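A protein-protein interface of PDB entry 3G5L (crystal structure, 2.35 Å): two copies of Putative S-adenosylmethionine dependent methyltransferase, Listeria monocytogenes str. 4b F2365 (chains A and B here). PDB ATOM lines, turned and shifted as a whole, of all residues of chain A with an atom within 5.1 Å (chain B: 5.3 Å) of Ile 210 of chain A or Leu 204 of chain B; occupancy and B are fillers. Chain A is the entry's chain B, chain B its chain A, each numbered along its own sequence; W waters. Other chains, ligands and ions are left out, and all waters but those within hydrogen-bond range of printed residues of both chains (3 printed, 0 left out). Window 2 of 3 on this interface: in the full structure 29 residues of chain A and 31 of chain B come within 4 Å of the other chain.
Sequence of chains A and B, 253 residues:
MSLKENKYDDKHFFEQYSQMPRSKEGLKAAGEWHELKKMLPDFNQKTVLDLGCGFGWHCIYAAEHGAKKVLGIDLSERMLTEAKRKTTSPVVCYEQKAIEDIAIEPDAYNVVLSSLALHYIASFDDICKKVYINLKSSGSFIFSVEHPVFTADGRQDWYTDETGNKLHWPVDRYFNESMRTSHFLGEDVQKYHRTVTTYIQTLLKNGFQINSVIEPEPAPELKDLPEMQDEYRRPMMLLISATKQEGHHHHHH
The side-chain hydroxyl (OG) of Ser 212 of chain A lies within hydrogen-bond range of the side-chain amide nitrogen (NE2) of Gln 201 of chain B (3.4 Å). The backbone NH (N) of Val 213 of chain A is in hydrogen-bond range of the side-chain amide oxygen (OE1) of Gln 201 of chain B (3.0 Å).
The side-chain amide nitrogen (NE2) of Gln 209 of chain A lies within hydrogen-bond range of the side-chain amide oxygen (OD1) of Asn 211 of chain A, 2.8 Å away. N of Asn 211 of chain A lies within hydrogen-bond range of O of Ser 241 of chain A, 2.9 Å away. The backbone carbonyl oxygen (O) of Ser 212 of chain A sits at hydrogen-bond distance from the backbone NH (N) of Ser 241 of chain A, 2.9 Å away.
CD1 of Ile 200 of chain B touches CD1 of Ile 200 of chain A (3.7 Å). CD1 of Leu 204 of chain A touches O of Ile 210 of chain B, 3.9 Å away. Ile 210 of chain A touches Leu 204 of chain B (O to CD2, 3.7 Å). Asn 211 of chain A touches Leu 204 of chain B (O to CD1, 3.4 Å). CD1 of Leu 204 of chain B touches N of Ser 212 of chain A, at 3.98 Å.
Ile 210 of chain A touches one residue of chain B. Printed residues of chain A within 4 Å of Leu 204 of chain B: Ile 210 (3.7 Å), Asn 211 (3.4 Å) and Ser 212 (3.98 Å). Of the printed residues of chain A, Ile 200 of chain B touches Ile 200 (3.7 Å). Of the printed residues of chain B, Val 213 of chain A touches Gln 201. Of the printed residues of chain A, Gln 201 of chain B touches Ser 212 and Val 213. Gly 207 of chain B touches none of the printed residues of chain A. Phe 208 of chain A touches none of the printed residues of chain B. The nearest printed residue of chain A that does not touch Leu 204 of chain B is Val 213 of chain A (4.7 Å).
Printed residues of chain B that touch a printed residue of chain A: Ile 200, Gln 201, Leu 204 and Ile 210. Hydrophobic or aromatic side chains of chain B that line the printed part of chain A: Ile 200 and Leu 204. Along chain A the printed residues that touch a printed residue of chain B span positions 200 to 213. Among the printed residues, no Asp or Glu carboxylate lies within 4 Å of a Lys or Arg side-chain nitrogen of the other chain.
Ile 200 of chain A touches its own counterpart, Ile 200 of chain B. Leu 204 of chain A touches Ile 210 of chain B, and with the chains exchanged Ile 210 of chain A touches Leu 204 of chain B. Of the 7 pairs that touch across the chains among the printed residues, 3 have their exchanged pair printed and touching as well.
Water W3 bridges O of Ile 210 of chain A and N of Ile 210 of chain B. Water W2 bridges O of Ile 210 of chain B and N of Ile 210 of chain A. Water W1 bridges the backbone carbonyl oxygen (O) of Asn 211 of chain A (2.8 Å) and the side-chain amide nitrogen (NE2) of Gln 201 of chain B (3.1 Å).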
ATOM      1  N   ILE A 200     -29.460  -4.148  23.460  1.00  0.00           N
ATOM      2  CA  ILE A 200     -29.012  -5.276  24.276  1.00  0.00           C
ATOM      3  C   ILE A 200     -30.142  -5.906  25.101  1.00  0.00           C
ATOM      4  O   ILE A 200     -30.313  -7.127  25.055  1.00  0.00           O
ATOM      5  CB  ILE A 200     -27.752  -4.932  25.109  1.00  0.00           C
ATOM      6  CG1 ILE A 200     -26.581  -4.630  24.168  1.00  0.00           C
ATOM      7  CG2 ILE A 200     -27.348  -6.085  26.025  1.00  0.00           C
ATOM      8  CD1 ILE A 200     -25.369  -4.102  24.871  1.00  0.00           C
ATOM      9  N   LEU A 203     -32.890  -7.909  22.963  1.00  0.00           N
ATOM     10  CA  LEU A 203     -32.351  -9.230  22.643  1.00  0.00           C
ATOM     11  C   LEU A 203     -32.463 -10.165  23.848  1.00  0.00           C
ATOM     12  O   LEU A 203     -32.994 -11.269  23.735  1.00  0.00           O
ATOM     13  CB  LEU A 203     -30.897  -9.123  22.186  1.00  0.00           C
ATOM     14  CG  LEU A 203     -30.691  -8.664  20.750  1.00  0.00           C
ATOM     15  CD1 LEU A 203     -29.329  -8.040  20.577  1.00  0.00           C
ATOM     16  CD2 LEU A 203     -30.886  -9.811  19.779  1.00  0.00           C
ATOM     17  N   LEU A 204     -32.002  -9.687  24.998  1.00  0.00           N
ATOM     18  CA  LEU A 204     -32.067 -10.437  26.251  1.00  0.00           C
ATOM     19  C   LEU A 204     -33.483 -10.844  26.681  1.00  0.00           C
ATOM     20  O   LEU A 204     -33.697 -11.993  27.078  1.00  0.00           O
ATOM     21  CB  LEU A 204     -31.376  -9.651  27.368  1.00  0.00           C
ATOM     22  CG  LEU A 204     -29.964  -9.970  27.884  1.00  0.00           C
ATOM     23  CD1 LEU A 204     -29.198 -11.043  27.121  1.00  0.00           C
ATOM     24  CD2 LEU A 204     -29.168  -8.684  27.960  1.00  0.00           C
ATOM     25  N   PHE A 208     -32.507 -14.183  23.700  1.00  0.00           N
ATOM     26  CA  PHE A 208     -31.182 -14.310  23.094  1.00  0.00           C
ATOM     27  C   PHE A 208     -30.065 -14.219  24.128  1.00  0.00           C
ATOM     28  O   PHE A 208     -30.213 -13.573  25.159  1.00  0.00           O
ATOM     29  CB  PHE A 208     -30.952 -13.257  22.007  1.00  0.00           C
ATOM     30  CG  PHE A 208     -31.795 -13.443  20.784  1.00  0.00           C
ATOM     31  CD1 PHE A 208     -31.392 -14.313  19.769  1.00  0.00           C
ATOM     32  CD2 PHE A 208     -32.985 -12.724  20.629  1.00  0.00           C
ATOM     33  CE1 PHE A 208     -32.169 -14.479  18.616  1.00  0.00           C
ATOM     34  CE2 PHE A 208     -33.770 -12.876  19.481  1.00  0.00           C
ATOM     35  CZ  PHE A 208     -33.360 -13.759  18.471  1.00  0.00           C
ATOM     36  N   GLN A 209     -28.950 -14.878  23.832  1.00  0.00           N
ATOM     37  CA  GLN A 209     -27.725 -14.764  24.609  1.00  0.00           C
ATOM     38  C   GLN A 209     -26.795 -13.842  23.836  1.00  0.00           C
ATOM     39  O   GLN A 209     -26.646 -13.995  22.629  1.00  0.00           O
ATOM     40  CB  GLN A 209     -27.058 -16.137  24.754  1.00  0.00           C
ATOM     41  CG  GLN A 209     -25.755 -16.138  25.561  1.00  0.00           C
ATOM     42  CD  GLN A 209     -24.651 -17.004  24.953  1.00  0.00           C
ATOM     43  OE1 GLN A 209     -24.904 -18.055  24.356  1.00  0.00           O
ATOM     44  NE2 GLN A 209     -23.410 -16.549  25.097  1.00  0.00           N
ATOM     45  N   ILE A 210     -26.173 -12.891  24.529  1.00  0.00           N
ATOM     46  CA  ILE A 210     -25.207 -11.986  23.916  1.00  0.00           C
ATOM     47  C   ILE A 210     -23.846 -12.699  23.789  1.00  0.00           C
ATOM     48  O   ILE A 210     -23.285 -13.132  24.794  1.00  0.00           O
ATOM     49  CB  ILE A 210     -25.067 -10.691  24.759  1.00  0.00           C
ATOM     50  CG1 ILE A 210     -26.415  -9.956  24.875  1.00  0.00           C
ATOM     51  CG2 ILE A 210     -23.975  -9.772  24.203  1.00  0.00           C
ATOM     52  CD1 ILE A 210     -27.103  -9.622  23.549  1.00  0.00           C
ATOM     53  N   ASN A 211     -23.331 -12.823  22.563  1.00  0.00           N
ATOM     54  CA  ASN A 211     -22.033 -13.467  22.313  1.00  0.00           C
ATOM     55  C   ASN A 211     -20.876 -12.497  22.058  1.00  0.00           C
ATOM     56  O   ASN A 211     -19.712 -12.823  22.323  1.00  0.00           O
ATOM     57  CB  ASN A 211     -22.113 -14.411  21.116  1.00  0.00           C
ATOM     58  CG  ASN A 211     -23.181 -15.463  21.267  1.00  0.00           C
ATOM     59  OD1 ASN A 211     -23.332 -16.070  22.323  1.00  0.00           O
ATOM     60  ND2 ASN A 211     -23.932 -15.689  20.198  1.00  0.00           N
ATOM     61  N   SER A 212     -21.204 -11.323  21.522  1.00  0.00           N
ATOM     62  CA  SER A 212     -20.216 -10.334  21.094  1.00  0.00           C
ATOM     63  C   SER A 212     -20.900  -8.998  20.843  1.00  0.00           C
ATOM     64  O   SER A 212     -21.954  -8.949  20.197  1.00  0.00           O
ATOM     65  CB  SER A 212     -19.501 -10.798  19.817  1.00  0.00           C
ATOM     66  OG  SER A 212     -18.421  -9.945  19.485  1.00  0.00           O
ATOM     67  N   VAL A 213     -20.316  -7.927  21.386  1.00  0.00           N
ATOM     68  CA  VAL A 213     -20.736  -6.548  21.083  1.00  0.00           C
ATOM     69  C   VAL A 213     -19.493  -5.740  20.697  1.00  0.00           C
ATOM     70  O   VAL A 213     -18.586  -5.566  21.508  1.00  0.00           O
ATOM     71  CB  VAL A 213     -21.482  -5.857  22.267  1.00  0.00           C
ATOM     72  CG1 VAL A 213     -21.863  -4.414  21.908  1.00  0.00           C
ATOM     73  CG2 VAL A 213     -22.749  -6.613  22.661  1.00  0.00           C
ATOM     74  N   ILE A 240     -23.722  -6.480  16.933  1.00  0.00           N
ATOM     75  CA  ILE A 240     -24.083  -7.442  17.967  1.00  0.00           C
ATOM     76  C   ILE A 240     -24.268  -8.845  17.368  1.00  0.00           C
ATOM     77  O   ILE A 240     -24.911  -9.002  16.329  1.00  0.00           O
ATOM     78  CB  ILE A 240     -25.358  -6.999  18.742  1.00  0.00           C
ATOM     79  CG1 ILE A 240     -25.137  -5.632  19.423  1.00  0.00           C
ATOM     80  CG2 ILE A 240     -25.763  -8.048  19.781  1.00  0.00           C
ATOM     81  CD1 ILE A 240     -26.367  -5.055  20.127  1.00  0.00           C
ATOM     82  N   SER A 241     -23.674  -9.846  18.018  1.00  0.00           N
ATOM     83  CA  SER A 241     -23.931 -11.255  17.718  1.00  0.00           C
ATOM     84  C   SER A 241     -24.666 -11.908  18.883  1.00  0.00           C
ATOM     85  O   SER A 241     -24.237 -11.805  20.037  1.00  0.00           O
ATOM     86  CB  SER A 241     -22.621 -11.995  17.450  1.00  0.00           C
ATOM     87  OG  SER A 241     -22.853 -13.356  17.130  1.00  0.00           O
ATOM     88  N   ALA A 242     -25.769 -12.582  18.575  1.00  0.00           N
ATOM     89  CA  ALA A 242     -26.611 -13.206  19.596  1.00  0.00           C
ATOM     90  C   ALA A 242     -27.036 -14.604  19.183  1.00  0.00           C
ATOM     91  O   ALA A 242     -27.160 -14.875  17.995  1.00  0.00           O
ATOM     92  CB  ALA A 242     -27.838 -12.338  19.880  1.00  0.00           C
ATOM     93  N   ILE B 200     -17.771  -4.963  27.694  1.00  0.00           N
ATOM     94  CA  ILE B 200     -18.550  -6.158  27.367  1.00  0.00           C
ATOM     95  C   ILE B 200     -17.665  -7.320  26.901  1.00  0.00           C
ATOM     96  O   ILE B 200     -17.814  -8.435  27.405  1.00  0.00           O
ATOM     97  CB  ILE B 200     -19.686  -5.848  26.351  1.00  0.00           C
ATOM     98  CG1 ILE B 200     -20.687  -4.868  26.969  1.00  0.00           C
ATOM     99  CG2 ILE B 200     -20.416  -7.130  25.915  1.00  0.00           C
ATOM    100  CD1 ILE B 200     -21.819  -4.446  26.019  1.00  0.00           C
ATOM    101  N   GLN B 201     -16.737  -7.052  25.975  1.00  0.00           N
ATOM    102  CA  GLN B 201     -15.834  -8.094  25.431  1.00  0.00           C
ATOM    103  C   GLN B 201     -14.858  -8.654  26.455  1.00  0.00           C
ATOM    104  O   GLN B 201     -14.525  -9.841  26.407  1.00  0.00           O
ATOM    105  CB  GLN B 201     -15.044  -7.597  24.208  1.00  0.00           C
ATOM    106  CG  GLN B 201     -15.907  -7.245  22.997  1.00  0.00           C
ATOM    107  CD  GLN B 201     -16.579  -8.455  22.394  1.00  0.00           C
ATOM    108  OE1 GLN B 201     -17.748  -8.725  22.662  1.00  0.00           O
ATOM    109  NE2 GLN B 201     -15.837  -9.199  21.588  1.00  0.00           N
ATOM    110  N   THR B 202     -14.413  -7.800  27.375  1.00  0.00           N
ATOM    111  CA  THR B 202     -13.536  -8.220  28.462  1.00  0.00           C
ATOM    112  C   THR B 202     -14.224  -9.204  29.401  1.00  0.00           C
ATOM    113  O   THR B 202     -13.636 -10.218  29.773  1.00  0.00           O
ATOM    114  CB  THR B 202     -12.956  -7.008  29.215  1.00  0.00           C
ATOM    115  OG1 THR B 202     -12.268  -6.179  28.269  1.00  0.00           O
ATOM    116  CG2 THR B 202     -11.973  -7.441  30.311  1.00  0.00           C
ATOM    117  N   LEU B 203     -15.472  -8.910  29.765  1.00  0.00           N
ATOM    118  CA  LEU B 203     -16.270  -9.847  30.545  1.00  0.00           C
ATOM    119  C   LEU B 203     -16.454 -11.190  29.821  1.00  0.00           C
ATOM    120  O   LEU B 203     -16.253 -12.241  30.422  1.00  0.00           O
ATOM    121  CB  LEU B 203     -17.621  -9.241  30.905  1.00  0.00           C
ATOM    122  CG  LEU B 203     -17.584  -8.178  31.993  1.00  0.00           C
ATOM    123  CD1 LEU B 203     -18.855  -7.355  31.945  1.00  0.00           C
ATOM    124  CD2 LEU B 203     -17.382  -8.808  33.365  1.00  0.00           C
ATOM    125  N   LEU B 204     -16.801 -11.135  28.535  1.00  0.00           N
ATOM    126  CA  LEU B 204     -17.086 -12.330  27.735  1.00  0.00           C
ATOM    127  C   LEU B 204     -15.870 -13.226  27.530  1.00  0.00           C
ATOM    128  O   LEU B 204     -15.996 -14.442  27.664  1.00  0.00           O
ATOM    129  CB  LEU B 204     -17.718 -11.967  26.374  1.00  0.00           C
ATOM    130  CG  LEU B 204     -19.165 -11.460  26.398  1.00  0.00           C
ATOM    131  CD1 LEU B 204     -19.511 -10.765  25.084  1.00  0.00           C
ATOM    132  CD2 LEU B 204     -20.163 -12.586  26.698  1.00  0.00           C
ATOM    133  N   LYS B 205     -14.705 -12.634  27.228  1.00  0.00           N
ATOM    134  CA  LYS B 205     -13.472 -13.406  27.026  1.00  0.00           C
ATOM    135  C   LYS B 205     -12.900 -13.964  28.335  1.00  0.00           C
ATOM    136  O   LYS B 205     -12.105 -14.908  28.324  1.00  0.00           O
ATOM    137  CB  LYS B 205     -12.417 -12.588  26.275  1.00  0.00           C
ATOM    138  CG  LYS B 205     -11.676 -11.564  27.112  1.00  0.00           C
ATOM    139  CD  LYS B 205     -10.508 -10.954  26.355  1.00  0.00           C
ATOM    140  CE  LYS B 205      -9.687 -10.048  27.265  1.00  0.00           C
ATOM    141  NZ  LYS B 205      -8.969 -10.824  28.316  1.00  0.00           N
ATOM    142  N   ASN B 206     -13.305 -13.372  29.459  1.00  0.00           N
ATOM    143  CA  ASN B 206     -12.897 -13.865  30.764  1.00  0.00           C
ATOM    144  C   ASN B 206     -13.833 -14.917  31.354  1.00  0.00           C
ATOM    145  O   ASN B 206     -13.630 -15.345  32.482  1.00  0.00           O
ATOM    146  CB  ASN B 206     -12.653 -12.716  31.739  1.00  0.00           C
ATOM    147  CG  ASN B 206     -11.319 -12.035  31.495  1.00  0.00           C
ATOM    148  OD1 ASN B 206     -10.265 -12.641  31.670  1.00  0.00           O
ATOM    149  ND2 ASN B 206     -11.359 -10.783  31.065  1.00  0.00           N
ATOM    150  N   GLY B 207     -14.846 -15.324  30.583  1.00  0.00           N
ATOM    151  CA  GLY B 207     -15.720 -16.440  30.954  1.00  0.00           C
ATOM    152  C   GLY B 207     -17.022 -16.054  31.639  1.00  0.00           C
ATOM    153  O   GLY B 207     -17.631 -16.874  32.317  1.00  0.00           O
ATOM    154  N   PHE B 208     -17.447 -14.804  31.473  1.00  0.00           N
ATOM    155  CA  PHE B 208     -18.715 -14.357  32.026  1.00  0.00           C
ATOM    156  C   PHE B 208     -19.797 -14.329  30.962  1.00  0.00           C
ATOM    157  O   PHE B 208     -19.516 -14.120  29.776  1.00  0.00           O
ATOM    158  CB  PHE B 208     -18.595 -12.961  32.635  1.00  0.00           C
ATOM    159  CG  PHE B 208     -17.761 -12.897  33.880  1.00  0.00           C
ATOM    160  CD1 PHE B 208     -18.325 -13.156  35.125  1.00  0.00           C
ATOM    161  CD2 PHE B 208     -16.416 -12.547  33.813  1.00  0.00           C
ATOM    162  CE1 PHE B 208     -17.562 -13.076  36.283  1.00  0.00           C
ATOM    163  CE2 PHE B 208     -15.645 -12.467  34.963  1.00  0.00           C
ATOM    164  CZ  PHE B 208     -16.222 -12.727  36.203  1.00  0.00           C
ATOM    165  N   GLN B 209     -21.035 -14.538  31.407  1.00  0.00           N
ATOM    166  CA  GLN B 209     -22.229 -14.408  30.575  1.00  0.00           C
ATOM    167  C   GLN B 209     -22.873 -13.068  30.917  1.00  0.00           C
ATOM    168  O   GLN B 209     -22.955 -12.713  32.086  1.00  0.00           O
ATOM    169  CB  GLN B 209     -23.206 -15.538  30.903  1.00  0.00           C
ATOM    170  CG  GLN B 209     -24.453 -15.615  30.047  1.00  0.00           C
ATOM    171  CD  GLN B 209     -25.696 -16.024  30.847  1.00  0.00           C
ATOM    172  OE1 GLN B 209     -26.700 -15.311  30.862  1.00  0.00           O
ATOM    173  NE2 GLN B 209     -25.625 -17.169  31.519  1.00  0.00           N
ATOM    174  N   ILE B 210     -23.333 -12.336  29.905  1.00  0.00           N
ATOM    175  CA  ILE B 210     -23.976 -11.039  30.111  1.00  0.00           C
ATOM    176  C   ILE B 210     -25.480 -11.208  30.411  1.00  0.00           C
ATOM    177  O   ILE B 210     -26.226 -11.693  29.571  1.00  0.00           O
ATOM    178  CB  ILE B 210     -23.770 -10.110  28.882  1.00  0.00           C
ATOM    179  CG1 ILE B 210     -22.271  -9.982  28.510  1.00  0.00           C
ATOM    180  CG2 ILE B 210     -24.450  -8.748  29.104  1.00  0.00           C
ATOM    181  CD1 ILE B 210     -21.460  -8.942  29.319  1.00  0.00           C
HETATM  182  O   HOH W   1     -17.082 -11.982  22.264  1.00  0.00           O
HETATM  183  O   HOH W   2     -26.292 -13.281  27.473  1.00  0.00           O
HETATM  184  O   HOH W   3     -23.530 -13.541  27.341  1.00  0.00           O
